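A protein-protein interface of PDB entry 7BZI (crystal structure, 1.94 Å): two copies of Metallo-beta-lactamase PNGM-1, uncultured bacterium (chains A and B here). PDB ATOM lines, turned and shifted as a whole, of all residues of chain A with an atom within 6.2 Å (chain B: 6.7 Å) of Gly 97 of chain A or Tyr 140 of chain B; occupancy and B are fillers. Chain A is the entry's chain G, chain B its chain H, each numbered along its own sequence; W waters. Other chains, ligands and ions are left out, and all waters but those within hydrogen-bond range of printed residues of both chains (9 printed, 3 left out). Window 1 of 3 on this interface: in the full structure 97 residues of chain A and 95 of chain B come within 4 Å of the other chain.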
ATOM      1  N   ILE A  65     -20.172  -3.302 -16.279  1.00  0.00           N
ATOM      2  CA  ILE A  65     -20.272  -4.767 -16.444  1.00  0.00           C
ATOM      3  C   ILE A  65     -19.798  -5.394 -15.131  1.00  0.00           C
ATOM      4  O   ILE A  65     -18.864  -6.172 -15.152  1.00  0.00           O
ATOM      5  CB  ILE A  65     -19.527  -5.205 -17.719  1.00  0.00           C
ATOM      6  CG1 ILE A  65     -19.773  -6.684 -18.024  1.00  0.00           C
ATOM      7  CG2 ILE A  65     -18.045  -4.863 -17.636  1.00  0.00           C
ATOM      8  CD1 ILE A  65     -19.382  -7.122 -19.414  1.00  0.00           C
ATOM      9  N   GLY A  66     -20.434  -4.978 -14.039  1.00  0.00           N
ATOM     10  CA  GLY A  66     -20.196  -5.447 -12.661  1.00  0.00           C
ATOM     11  C   GLY A  66     -20.334  -6.959 -12.516  1.00  0.00           C
ATOM     12  O   GLY A  66     -20.930  -7.634 -13.392  1.00  0.00           O
ATOM     13  N   SER A  67     -19.760  -7.484 -11.434  1.00  0.00           N
ATOM     14  CA  SER A  67     -19.783  -8.918 -11.069  1.00  0.00           C
ATOM     15  C   SER A  67     -21.230  -9.417 -11.072  1.00  0.00           C
ATOM     16  O   SER A  67     -22.077  -8.767 -10.450  1.00  0.00           O
ATOM     17  CB  SER A  67     -19.101  -9.122  -9.750  1.00  0.00           C
ATOM     18  OG  SER A  67     -17.805  -8.524  -9.784  1.00  0.00           O
ATOM     19  N   GLY A  68     -21.503 -10.490 -11.820  1.00  0.00           N
ATOM     20  CA  GLY A  68     -22.814 -11.157 -11.851  1.00  0.00           C
ATOM     21  C   GLY A  68     -23.655 -10.774 -13.047  1.00  0.00           C
ATOM     22  O   GLY A  68     -24.602 -11.485 -13.300  1.00  0.00           O
ATOM     23  N   LEU A  91     -13.932   2.071 -11.536  1.00  0.00           N
ATOM     24  CA  LEU A  91     -13.091   0.850 -11.646  1.00  0.00           C
ATOM     25  C   LEU A  91     -13.344  -0.079 -10.448  1.00  0.00           C
ATOM     26  O   LEU A  91     -12.562  -1.027 -10.259  1.00  0.00           O
ATOM     27  CB  LEU A  91     -11.630   1.270 -11.822  1.00  0.00           C
ATOM     28  CG  LEU A  91     -11.297   1.835 -13.205  1.00  0.00           C
ATOM     29  CD1 LEU A  91      -9.880   2.393 -13.259  1.00  0.00           C
ATOM     30  CD2 LEU A  91     -11.467   0.772 -14.274  1.00  0.00           C
ATOM     31  N   HIS A  92     -14.469   0.108  -9.753  1.00  0.00           N
ATOM     32  CA  HIS A  92     -14.978  -0.833  -8.722  1.00  0.00           C
ATOM     33  C   HIS A  92     -15.177  -2.209  -9.348  1.00  0.00           C
ATOM     34  O   HIS A  92     -15.573  -2.271 -10.550  1.00  0.00           O
ATOM     35  CB  HIS A  92     -16.302  -0.383  -8.133  1.00  0.00           C
ATOM     36  CG  HIS A  92     -16.202   0.553  -6.981  1.00  0.00           C
ATOM     37  ND1 HIS A  92     -16.828   1.786  -6.979  1.00  0.00           N
ATOM     38  CD2 HIS A  92     -15.626   0.421  -5.773  1.00  0.00           C
ATOM     39  CE1 HIS A  92     -16.623   2.364  -5.810  1.00  0.00           C
ATOM     40  NE2 HIS A  92     -15.883   1.554  -5.057  1.00  0.00           N
ATOM     41  N   THR A  93     -14.970  -3.263  -8.549  1.00  0.00           N
ATOM     42  CA  THR A  93     -15.250  -4.671  -8.944  1.00  0.00           C
ATOM     43  C   THR A  93     -16.704  -4.764  -9.406  1.00  0.00           C
ATOM     44  O   THR A  93     -16.951  -5.374 -10.466  1.00  0.00           O
ATOM     45  CB  THR A  93     -14.921  -5.663  -7.815  1.00  0.00           C
ATOM     46  OG1 THR A  93     -15.950  -5.604  -6.822  1.00  0.00           O
ATOM     47  CG2 THR A  93     -13.573  -5.374  -7.184  1.00  0.00           C
ATOM     48  N   ASP A  94     -17.616  -4.105  -8.691  1.00  0.00           N
ATOM     49  CA  ASP A  94     -19.072  -4.207  -8.964  1.00  0.00           C
ATOM     50  C   ASP A  94     -19.456  -3.279 -10.128  1.00  0.00           C
ATOM     51  O   ASP A  94     -20.665  -3.179 -10.383  1.00  0.00           O
ATOM     52  CB  ASP A  94     -19.893  -3.991  -7.690  1.00  0.00           C
ATOM     53  CG  ASP A  94     -19.910  -2.579  -7.126  1.00  0.00           C
ATOM     54  OD1 ASP A  94     -18.885  -1.869  -7.278  1.00  0.00           O
ATOM     55  OD2 ASP A  94     -20.944  -2.204  -6.503  1.00  0.00           O
ATOM     56  N   HIS A  95     -18.491  -2.695 -10.864  1.00  0.00           N
ATOM     57  CA  HIS A  95     -18.761  -1.896 -12.096  1.00  0.00           C
ATOM     58  C   HIS A  95     -18.003  -2.452 -13.308  1.00  0.00           C
ATOM     59  O   HIS A  95     -18.379  -2.070 -14.432  1.00  0.00           O
ATOM     60  CB  HIS A  95     -18.469  -0.409 -11.847  1.00  0.00           C
ATOM     61  CG  HIS A  95     -19.474   0.253 -10.954  1.00  0.00           C
ATOM     62  ND1 HIS A  95     -20.529   0.973 -11.449  1.00  0.00           N
ATOM     63  CD2 HIS A  95     -19.619   0.293  -9.608  1.00  0.00           C
ATOM     64  CE1 HIS A  95     -21.256   1.444 -10.448  1.00  0.00           C
ATOM     65  NE2 HIS A  95     -20.731   1.046  -9.317  1.00  0.00           N
ATOM     66  N   TRP A  96     -17.003  -3.329 -13.134  1.00  0.00           N
ATOM     67  CA  TRP A  96     -16.310  -3.939 -14.305  1.00  0.00           C
ATOM     68  C   TRP A  96     -15.811  -5.371 -14.038  1.00  0.00           C
ATOM     69  O   TRP A  96     -15.259  -5.958 -14.991  1.00  0.00           O
ATOM     70  CB  TRP A  96     -15.203  -3.004 -14.843  1.00  0.00           C
ATOM     71  CG  TRP A  96     -13.906  -2.993 -14.096  1.00  0.00           C
ATOM     72  CD1 TRP A  96     -13.672  -2.486 -12.854  1.00  0.00           C
ATOM     73  CD2 TRP A  96     -12.635  -3.463 -14.580  1.00  0.00           C
ATOM     74  NE1 TRP A  96     -12.351  -2.625 -12.529  1.00  0.00           N
ATOM     75  CE2 TRP A  96     -11.699  -3.245 -13.556  1.00  0.00           C
ATOM     76  CE3 TRP A  96     -12.207  -4.073 -15.762  1.00  0.00           C
ATOM     77  CZ2 TRP A  96     -10.360  -3.603 -13.682  1.00  0.00           C
ATOM     78  CZ3 TRP A  96     -10.883  -4.433 -15.887  1.00  0.00           C
ATOM     79  CH2 TRP A  96      -9.972  -4.200 -14.857  1.00  0.00           C
ATOM     80  N   GLY A  97     -16.140  -5.970 -12.889  1.00  0.00           N
ATOM     81  CA  GLY A  97     -15.805  -7.378 -12.552  1.00  0.00           C
ATOM     82  C   GLY A  97     -16.053  -8.368 -13.691  1.00  0.00           C
ATOM     83  O   GLY A  97     -15.211  -9.248 -13.873  1.00  0.00           O
ATOM     84  N   ASP A  98     -17.149  -8.249 -14.458  1.00  0.00           N
ATOM     85  CA  ASP A  98     -17.519  -9.273 -15.479  1.00  0.00           C
ATOM     86  C   ASP A  98     -16.952  -8.929 -16.850  1.00  0.00           C
ATOM     87  O   ASP A  98     -17.175  -9.710 -17.770  1.00  0.00           O
ATOM     88  CB  ASP A  98     -19.021  -9.562 -15.548  1.00  0.00           C
ATOM     89  CG  ASP A  98     -19.413 -10.725 -14.640  1.00  0.00           C
ATOM     90  OD1 ASP A  98     -18.488 -11.268 -13.945  1.00  0.00           O
ATOM     91  OD2 ASP A  98     -20.627 -11.089 -14.619  1.00  0.00           O
ATOM     92  N   LEU A  99     -16.152  -7.881 -16.981  1.00  0.00           N
ATOM     93  CA  LEU A  99     -15.435  -7.672 -18.265  1.00  0.00           C
ATOM     94  C   LEU A  99     -14.743  -8.986 -18.660  1.00  0.00           C
ATOM     95  O   LEU A  99     -14.797  -9.366 -19.841  1.00  0.00           O
ATOM     96  CB  LEU A  99     -14.439  -6.524 -18.105  1.00  0.00           C
ATOM     97  CG  LEU A  99     -13.591  -6.243 -19.344  1.00  0.00           C
ATOM     98  CD1 LEU A  99     -14.473  -5.928 -20.545  1.00  0.00           C
ATOM     99  CD2 LEU A  99     -12.611  -5.115 -19.088  1.00  0.00           C
ATOM    100  N   VAL A 100     -14.119  -9.678 -17.700  1.00  0.00           N
ATOM    101  CA  VAL A 100     -13.269 -10.871 -17.974  1.00  0.00           C
ATOM    102  C   VAL A 100     -14.156 -12.013 -18.504  1.00  0.00           C
ATOM    103  O   VAL A 100     -13.778 -12.650 -19.518  1.00  0.00           O
ATOM    104  CB  VAL A 100     -12.439 -11.239 -16.720  1.00  0.00           C
ATOM    105  CG1 VAL A 100     -13.255 -11.873 -15.604  1.00  0.00           C
ATOM    106  CG2 VAL A 100     -11.275 -12.128 -17.088  1.00  0.00           C
ATOM    107  N   SER A 101     -15.337 -12.201 -17.906  1.00  0.00           N
ATOM    108  CA  SER A 101     -16.375 -13.194 -18.290  1.00  0.00           C
ATOM    109  C   SER A 101     -16.798 -12.963 -19.752  1.00  0.00           C
ATOM    110  O   SER A 101     -16.856 -13.932 -20.547  1.00  0.00           O
ATOM    111  CB  SER A 101     -17.548 -13.116 -17.334  1.00  0.00           C
ATOM    112  OG  SER A 101     -18.374 -14.262 -17.449  1.00  0.00           O
ATOM    113  N   ALA A 132      -5.413  -0.721 -15.328  1.00  0.00           N
ATOM    114  CA  ALA A 132      -6.395  -1.718 -14.841  1.00  0.00           C
ATOM    115  C   ALA A 132      -6.546  -2.836 -15.879  1.00  0.00           C
ATOM    116  O   ALA A 132      -6.406  -4.016 -15.501  1.00  0.00           O
ATOM    117  CB  ALA A 132      -7.706  -1.057 -14.528  1.00  0.00           C
ATOM    118  N   HIS A 135      -3.315  -4.916 -16.562  1.00  0.00           N
ATOM    119  CA  HIS A 135      -3.012  -5.862 -15.456  1.00  0.00           C
ATOM    120  C   HIS A 135      -4.071  -6.964 -15.393  1.00  0.00           C
ATOM    121  O   HIS A 135      -3.732  -8.074 -14.927  1.00  0.00           O
ATOM    122  CB  HIS A 135      -2.765  -5.104 -14.157  1.00  0.00           C
ATOM    123  CG  HIS A 135      -1.392  -4.539 -14.175  1.00  0.00           C
ATOM    124  ND1 HIS A 135      -0.275  -5.357 -14.227  1.00  0.00           N
ATOM    125  CD2 HIS A 135      -0.944  -3.270 -14.279  1.00  0.00           C
ATOM    126  CE1 HIS A 135       0.809  -4.607 -14.289  1.00  0.00           C
ATOM    127  NE2 HIS A 135       0.423  -3.325 -14.312  1.00  0.00           N
ATOM    128  N   MET A 136      -5.279  -6.704 -15.901  1.00  0.00           N
ATOM    129  CA  MET A 136      -6.351  -7.729 -15.964  1.00  0.00           C
ATOM    130  C   MET A 136      -5.918  -8.794 -16.971  1.00  0.00           C
ATOM    131  O   MET A 136      -6.085  -9.975 -16.668  1.00  0.00           O
ATOM    132  CB  MET A 136      -7.697  -7.128 -16.377  1.00  0.00           C
ATOM    133  CG  MET A 136      -8.869  -8.050 -16.130  1.00  0.00           C
ATOM    134  SD  MET A 136     -10.039  -7.996 -17.511  1.00  0.00           S
ATOM    135  CE  MET A 136      -9.143  -9.001 -18.695  1.00  0.00           C
ATOM    136  N   TYR A 140      -5.011 -12.822 -16.314  1.00  0.00           N
ATOM    137  CA  TYR A 140      -5.624 -13.983 -16.997  1.00  0.00           C
ATOM    138  C   TYR A 140      -4.688 -14.470 -18.111  1.00  0.00           C
ATOM    139  O   TYR A 140      -5.158 -15.068 -19.089  1.00  0.00           O
ATOM    140  CB  TYR A 140      -7.068 -13.628 -17.373  1.00  0.00           C
ATOM    141  CG  TYR A 140      -7.967 -13.462 -16.173  1.00  0.00           C
ATOM    142  CD1 TYR A 140      -8.563 -14.564 -15.578  1.00  0.00           C
ATOM    143  CD2 TYR A 140      -8.218 -12.219 -15.624  1.00  0.00           C
ATOM    144  CE1 TYR A 140      -9.389 -14.436 -14.472  1.00  0.00           C
ATOM    145  CE2 TYR A 140      -9.041 -12.069 -14.516  1.00  0.00           C
ATOM    146  CZ  TYR A 140      -9.618 -13.186 -13.928  1.00  0.00           C
ATOM    147  OH  TYR A 140     -10.444 -13.062 -12.842  1.00  0.00           O
ATOM    148  N   SER B  67     -16.758 -17.128 -12.333  1.00  0.00           N
ATOM    149  CA  SER B  67     -17.658 -15.996 -12.651  1.00  0.00           C
ATOM    150  C   SER B  67     -19.089 -16.406 -12.334  1.00  0.00           C
ATOM    151  O   SER B  67     -19.529 -17.510 -12.817  1.00  0.00           O
ATOM    152  CB  SER B  67     -17.517 -15.578 -14.070  1.00  0.00           C
ATOM    153  OG  SER B  67     -16.190 -15.167 -14.310  1.00  0.00           O
ATOM    154  N   GLY B  97     -12.811 -16.344 -11.705  1.00  0.00           N
ATOM    155  CA  GLY B  97     -13.400 -15.038 -12.057  1.00  0.00           C
ATOM    156  C   GLY B  97     -14.036 -14.319 -10.878  1.00  0.00           C
ATOM    157  O   GLY B  97     -13.909 -13.095 -10.842  1.00  0.00           O
ATOM    158  N   ASP B  98     -14.680 -15.005  -9.922  1.00  0.00           N
ATOM    159  CA  ASP B  98     -15.338 -14.296  -8.781  1.00  0.00           C
ATOM    160  C   ASP B  98     -14.419 -14.116  -7.566  1.00  0.00           C
ATOM    161  O   ASP B  98     -14.915 -13.589  -6.545  1.00  0.00           O
ATOM    162  CB  ASP B  98     -16.667 -14.933  -8.371  1.00  0.00           C
ATOM    163  CG  ASP B  98     -17.832 -14.275  -9.091  1.00  0.00           C
ATOM    164  OD1 ASP B  98     -17.560 -13.528 -10.094  1.00  0.00           O
ATOM    165  OD2 ASP B  98     -19.011 -14.505  -8.670  1.00  0.00           O
ATOM    166  N   VAL B 100     -12.202 -11.847  -7.183  1.00  0.00           N
ATOM    167  CA  VAL B 100     -12.256 -10.378  -6.978  1.00  0.00           C
ATOM    168  C   VAL B 100     -13.542  -9.964  -6.241  1.00  0.00           C
ATOM    169  O   VAL B 100     -13.447  -9.064  -5.413  1.00  0.00           O
ATOM    170  CB  VAL B 100     -12.091  -9.633  -8.314  1.00  0.00           C
ATOM    171  CG1 VAL B 100     -13.174 -10.001  -9.314  1.00  0.00           C
ATOM    172  CG2 VAL B 100     -12.033  -8.130  -8.075  1.00  0.00           C
ATOM    173  N   TRP B 103     -13.134 -11.000  -2.675  1.00  0.00           N
ATOM    174  CA  TRP B 103     -12.112 -10.056  -2.164  1.00  0.00           C
ATOM    175  C   TRP B 103     -12.758  -8.712  -1.794  1.00  0.00           C
ATOM    176  O   TRP B 103     -12.690  -8.289  -0.626  1.00  0.00           O
ATOM    177  CB  TRP B 103     -11.030  -9.909  -3.233  1.00  0.00           C
ATOM    178  CG  TRP B 103     -10.015  -8.851  -2.956  1.00  0.00           C
ATOM    179  CD1 TRP B 103      -9.078  -8.854  -1.966  1.00  0.00           C
ATOM    180  CD2 TRP B 103      -9.854  -7.613  -3.671  1.00  0.00           C
ATOM    181  NE1 TRP B 103      -8.327  -7.718  -2.039  1.00  0.00           N
ATOM    182  CE2 TRP B 103      -8.774  -6.936  -3.071  1.00  0.00           C
ATOM    183  CE3 TRP B 103     -10.494  -7.028  -4.766  1.00  0.00           C
ATOM    184  CZ2 TRP B 103      -8.324  -5.697  -3.524  1.00  0.00           C
ATOM    185  CZ3 TRP B 103     -10.037  -5.815  -5.228  1.00  0.00           C
ATOM    186  CH2 TRP B 103      -8.973  -5.152  -4.609  1.00  0.00           C
ATOM    187  N   HIS B 135      -1.206  -9.731 -10.320  1.00  0.00           N
ATOM    188  CA  HIS B 135      -1.700  -8.897 -11.444  1.00  0.00           C
ATOM    189  C   HIS B 135      -3.206  -8.634 -11.277  1.00  0.00           C
ATOM    190  O   HIS B 135      -3.634  -7.562 -11.703  1.00  0.00           O
ATOM    191  CB  HIS B 135      -1.243  -9.506 -12.766  1.00  0.00           C
ATOM    192  CG  HIS B 135       0.199  -9.214 -13.019  1.00  0.00           C
ATOM    193  ND1 HIS B 135       0.653  -7.938 -13.295  1.00  0.00           N
ATOM    194  CD2 HIS B 135       1.297  -9.997 -12.998  1.00  0.00           C
ATOM    195  CE1 HIS B 135       1.962  -7.957 -13.459  1.00  0.00           C
ATOM    196  NE2 HIS B 135       2.379  -9.204 -13.274  1.00  0.00           N
ATOM    197  N   MET B 136      -3.961  -9.514 -10.603  1.00  0.00           N
ATOM    198  CA  MET B 136      -5.393  -9.266 -10.312  1.00  0.00           C
ATOM    199  C   MET B 136      -5.489  -8.052  -9.375  1.00  0.00           C
ATOM    200  O   MET B 136      -6.281  -7.141  -9.647  1.00  0.00           O
ATOM    201  CB  MET B 136      -6.058 -10.483  -9.665  1.00  0.00           C
ATOM    202  CG  MET B 136      -7.564 -10.358  -9.540  1.00  0.00           C
ATOM    203  SD  MET B 136      -8.180 -11.151  -8.038  1.00  0.00           S
ATOM    204  CE  MET B 136      -7.830  -9.842  -6.870  1.00  0.00           C
ATOM    205  N   LEU B 137      -4.651  -8.005  -8.342  1.00  0.00           N
ATOM    206  CA  LEU B 137      -4.675  -6.924  -7.335  1.00  0.00           C
ATOM    207  C   LEU B 137      -4.246  -5.597  -7.973  1.00  0.00           C
ATOM    208  O   LEU B 137      -4.789  -4.575  -7.565  1.00  0.00           O
ATOM    209  CB  LEU B 137      -3.774  -7.309  -6.164  1.00  0.00           C
ATOM    210  CG  LEU B 137      -4.379  -8.297  -5.169  1.00  0.00           C
ATOM    211  CD1 LEU B 137      -3.315  -8.797  -4.211  1.00  0.00           C
ATOM    212  CD2 LEU B 137      -5.524  -7.656  -4.393  1.00  0.00           C
ATOM    213  N   LYS B 138      -3.309  -5.607  -8.916  1.00  0.00           N
ATOM    214  CA  LYS B 138      -2.914  -4.389  -9.677  1.00  0.00           C
ATOM    215  C   LYS B 138      -4.084  -3.964 -10.580  1.00  0.00           C
ATOM    216  O   LYS B 138      -4.458  -2.790 -10.548  1.00  0.00           O
ATOM    217  CB  LYS B 138      -1.683  -4.654 -10.551  1.00  0.00           C
ATOM    218  CG  LYS B 138      -0.401  -4.937  -9.787  1.00  0.00           C
ATOM    219  CD  LYS B 138       0.672  -5.572 -10.662  1.00  0.00           C
ATOM    220  CE  LYS B 138       1.886  -6.001  -9.866  1.00  0.00           C
ATOM    221  NZ  LYS B 138       2.529  -4.829  -9.237  1.00  0.00           N
ATOM    222  N   ALA B 139      -4.640  -4.913 -11.343  1.00  0.00           N
ATOM    223  CA  ALA B 139      -5.853  -4.710 -12.165  1.00  0.00           C
ATOM    224  C   ALA B 139      -6.875  -3.902 -11.361  1.00  0.00           C
ATOM    225  O   ALA B 139      -7.383  -2.941 -11.950  1.00  0.00           O
ATOM    226  CB  ALA B 139      -6.417  -6.017 -12.650  1.00  0.00           C
ATOM    227  N   TYR B 140      -7.121  -4.232 -10.080  1.00  0.00           N
ATOM    228  CA  TYR B 140      -8.152  -3.567  -9.228  1.00  0.00           C
ATOM    229  C   TYR B 140      -7.512  -2.602  -8.236  1.00  0.00           C
ATOM    230  O   TYR B 140      -8.037  -2.439  -7.145  1.00  0.00           O
ATOM    231  CB  TYR B 140      -9.039  -4.584  -8.500  1.00  0.00           C
ATOM    232  CG  TYR B 140      -9.897  -5.346  -9.467  1.00  0.00           C
ATOM    233  CD1 TYR B 140     -11.123  -4.842  -9.853  1.00  0.00           C
ATOM    234  CD2 TYR B 140      -9.435  -6.491 -10.097  1.00  0.00           C
ATOM    235  CE1 TYR B 140     -11.896  -5.478 -10.807  1.00  0.00           C
ATOM    236  CE2 TYR B 140     -10.187  -7.134 -11.066  1.00  0.00           C
ATOM    237  CZ  TYR B 140     -11.430  -6.629 -11.404  1.00  0.00           C
ATOM    238  OH  TYR B 140     -12.206  -7.233 -12.337  1.00  0.00           O
ATOM    239  N   ASN B 141      -6.425  -1.939  -8.623  1.00  0.00           N
ATOM    240  CA  ASN B 141      -5.653  -1.044  -7.733  1.00  0.00           C
ATOM    241  C   ASN B 141      -6.484   0.199  -7.377  1.00  0.00           C
ATOM    242  O   ASN B 141      -6.370   0.652  -6.229  1.00  0.00           O
ATOM    243  CB  ASN B 141      -4.316  -0.645  -8.364  1.00  0.00           C
ATOM    244  CG  ASN B 141      -3.465   0.112  -7.377  1.00  0.00           C
ATOM    245  OD1 ASN B 141      -3.172  -0.418  -6.323  1.00  0.00           O
ATOM    246  ND2 ASN B 141      -3.146   1.366  -7.652  1.00  0.00           N
ATOM    247  N   TRP B 142      -7.310   0.723  -8.296  1.00  0.00           N
ATOM    248  CA  TRP B 142      -8.192   1.882  -7.972  1.00  0.00           C
ATOM    249  C   TRP B 142      -9.110   1.457  -6.829  1.00  0.00           C
ATOM    250  O   TRP B 142      -9.217   2.180  -5.828  1.00  0.00           O
ATOM    251  CB  TRP B 142      -9.003   2.393  -9.172  1.00  0.00           C
ATOM    252  CG  TRP B 142      -9.866   3.558  -8.791  1.00  0.00           C
ATOM    253  CD1 TRP B 142      -9.523   4.875  -8.844  1.00  0.00           C
ATOM    254  CD2 TRP B 142     -11.204   3.515  -8.254  1.00  0.00           C
ATOM    255  NE1 TRP B 142     -10.528   5.649  -8.334  1.00  0.00           N
ATOM    256  CE2 TRP B 142     -11.592   4.851  -8.013  1.00  0.00           C
ATOM    257  CE3 TRP B 142     -12.126   2.491  -7.998  1.00  0.00           C
ATOM    258  CZ2 TRP B 142     -12.834   5.185  -7.478  1.00  0.00           C
ATOM    259  CZ3 TRP B 142     -13.363   2.816  -7.490  1.00  0.00           C
ATOM    260  CH2 TRP B 142     -13.704   4.148  -7.219  1.00  0.00           C
ATOM    261  N   ASP B 143      -9.717   0.289  -6.973  1.00  0.00           N
ATOM    262  CA  ASP B 143     -10.685  -0.210  -5.976  1.00  0.00           C
ATOM    263  C   ASP B 143      -9.939  -0.386  -4.658  1.00  0.00           C
ATOM    264  O   ASP B 143     -10.464   0.051  -3.609  1.00  0.00           O
ATOM    265  CB  ASP B 143     -11.356  -1.497  -6.463  1.00  0.00           C
ATOM    266  CG  ASP B 143     -12.488  -1.949  -5.560  1.00  0.00           C
ATOM    267  OD1 ASP B 143     -13.299  -1.098  -5.164  1.00  0.00           O
ATOM    268  OD2 ASP B 143     -12.506  -3.149  -5.211  1.00  0.00           O
ATOM    269  N   TYR B 144      -8.748  -0.995  -4.712  1.00  0.00           N
ATOM    270  CA  TYR B 144      -7.921  -1.279  -3.508  1.00  0.00           C
ATOM    271  C   TYR B 144      -7.608   0.034  -2.790  1.00  0.00           C
ATOM    272  O   TYR B 144      -7.819   0.147  -1.564  1.00  0.00           O
ATOM    273  CB  TYR B 144      -6.620  -2.005  -3.863  1.00  0.00           C
ATOM    274  CG  TYR B 144      -5.712  -2.225  -2.677  1.00  0.00           C
ATOM    275  CD1 TYR B 144      -6.058  -3.111  -1.671  1.00  0.00           C
ATOM    276  CD2 TYR B 144      -4.529  -1.516  -2.542  1.00  0.00           C
ATOM    277  CE1 TYR B 144      -5.250  -3.311  -0.567  1.00  0.00           C
ATOM    278  CE2 TYR B 144      -3.700  -1.704  -1.448  1.00  0.00           C
ATOM    279  CZ  TYR B 144      -4.072  -2.595  -0.455  1.00  0.00           C
ATOM    280  OH  TYR B 144      -3.273  -2.777   0.625  1.00  0.00           O
ATOM    281  N   MET B 145      -7.025   0.974  -3.533  1.00  0.00           N
ATOM    282  CA  MET B 145      -6.459   2.203  -2.937  1.00  0.00           C
ATOM    283  C   MET B 145      -7.615   3.005  -2.322  1.00  0.00           C
ATOM    284  O   MET B 145      -7.513   3.313  -1.123  1.00  0.00           O
ATOM    285  CB  MET B 145      -5.647   3.005  -3.966  1.00  0.00           C
ATOM    286  CG  MET B 145      -4.272   2.375  -4.284  1.00  0.00           C
ATOM    287  SD  MET B 145      -3.274   1.936  -2.823  1.00  0.00           S
ATOM    288  CE  MET B 145      -2.608   3.542  -2.389  1.00  0.00           C
ATOM    289  N   ARG B 147     -10.698   2.028  -1.429  1.00  0.00           N
ATOM    290  CA  ARG B 147     -11.358   1.311  -0.299  1.00  0.00           C
ATOM    291  C   ARG B 147     -10.495   1.391   0.963  1.00  0.00           C
ATOM    292  O   ARG B 147     -11.083   1.502   2.073  1.00  0.00           O
ATOM    293  CB  ARG B 147     -11.668  -0.153  -0.631  1.00  0.00           C
ATOM    294  CG  ARG B 147     -12.432  -0.853   0.482  1.00  0.00           C
ATOM    295  CD  ARG B 147     -13.129  -2.151   0.089  1.00  0.00           C
ATOM    296  NE  ARG B 147     -14.093  -2.018  -1.006  1.00  0.00           N
ATOM    297  CZ  ARG B 147     -13.889  -2.421  -2.259  1.00  0.00           C
ATOM    298  NH1 ARG B 147     -12.737  -2.984  -2.606  1.00  0.00           N
ATOM    299  NH2 ARG B 147     -14.836  -2.249  -3.165  1.00  0.00           N
HETATM  300  O   HOH W   1     -13.393   1.541  -3.415  1.00  0.00           O
HETATM  301  O   HOH W   2     -16.143 -12.692 -13.904  1.00  0.00           O
HETATM  302  O   HOH W   3     -20.900 -12.576  -9.386  1.00  0.00           O
HETATM  303  O   HOH W   4     -16.397 -10.755 -10.541  1.00  0.00           O
HETATM  304  O   HOH W   5     -16.163  -3.183  -5.406  1.00  0.00           O
HETATM  305  O   HOH W   6     -10.038  -1.176  -9.526  1.00  0.00           O
HETATM  306  O   HOH W   7     -19.270 -12.661 -11.854  1.00  0.00           O
HETATM  307  O   HOH W   8     -10.898 -12.848  -9.920  1.00  0.00           O
HETATM  308  O   HOH W   9     -14.204 -10.942 -12.147  1.00  0.00           O
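Gly 97 of chain A touches just one residue of chain B: Tyr 140.
Of chain A, only Thr 93 (3.7 Å), Trp 96 (3.4 Å) and Gly 97 (3.6 Å) come within 4 Å of Tyr 140 of chain B.
Of the printed residues of chain B, Trp 96 of chain A touches Ala 139 and Tyr 140.
Of the printed residues of chain B, His 135 of chain A touches His 135 (2.9 Å), Lys 138 (3.6 Å) and Ala 139 (3.4 Å).
Of the printed residues of chain A, Arg 147 of chain B touches His 92 (3.8 Å).
The nearest residue of chain B that does not touch Gly 97 of chain A is Val 100 of chain B (4.9 Å).
The nearest residue of chain A that does not touch Tyr 140 of chain B is Leu 91 of chain A (4.1 Å).
The nearest printed residue of chain B that does not touch Trp 96 of chain A is Asp 143 of chain B (6.2 Å).
Among the printed residues, merely in contact across the chains: Leu 91 of chain A with Trp 142 of chain B (3.8 Å), His 92 of chain A with Trp 142 of chain B (3.7 Å), His 92 of chain A with Asp 143 of chain B (2.8 Å), His 92 of chain A with Arg 147 of chain B (3.8 Å), Thr 93 of chain A with Val 100 of chain B (3.3 Å), Thr 93 of chain A with Tyr 140 of chain B (3.7 Å), Thr 93 of chain A with Asp 143 of chain B (3.2 Å), Trp 96 of chain A with Ala 139 of chain B (3.5 Å), Trp 96 of chain A with Tyr 140 of chain B (3.4 Å), Gly 97 of chain A with Tyr 140 of chain B (3.6 Å), Ser 101 of chain A with Ser 67 of chain B (3.7 Å), Ala 132 of chain A with Ala 139 of chain B (3.2 Å), His 135 of chain A with Lys 138 of chain B (3.6 Å), His 135 of chain A with Ala 139 of chain B (3.4 Å), Met 136 of chain A with Ala 139 of chain B (3.5 Å) and Tyr 140 of chain A with Gly 97 of chain B (3.6 Å).
Water W9 bridges the backbone carbonyl oxygen (O) of Gly 97 of chain B and the backbone carbonyl oxygen (O) of Gly 97 of chain A.
Gly 97 of chain A touches Tyr 140 of chain B, and with the chains exchanged Tyr 140 of chain A touches Gly 97 of chain B.
His 135 of chain B touches its own counterpart, His 135 of chain A.
Of the 17 pairs that touch across the chains among the printed residues, 3 have their exchanged pair printed and touching as well.
Printed residues of chain B that touch a printed residue of chain A: Ser 67, Gly 97, Val 100, His 135, Lys 138, Ala 139, Tyr 140, Trp 142, Asp 143 and Arg 147.
Among the printed residues, 17 pairs touch across the chains.
Among the printed residues, no Asp or Glu carboxylate lies within 4 Å of a Lys or Arg side-chain nitrogen of the other chain.
A ring nitrogen (ND1) of His 135 of chain A is in hydrogen-bond range of a ring nitrogen (ND1) of His 135 of chain B (2.9 Å).
OG of Ser 67 of chain A sits at hydrogen-bond distance from O of Thr 93 of chain A, at 3.3 Å.
NH1 of Arg 147 of chain B lies within salt-bridge range of OD2 of Asp 143 of chain B (2.6 Å).
The backbone carbonyl oxygen (O) of Leu 91 of chain A sits at hydrogen-bond distance from the indole nitrogen (NE1) of Trp 96 of chain A (2.8 Å).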
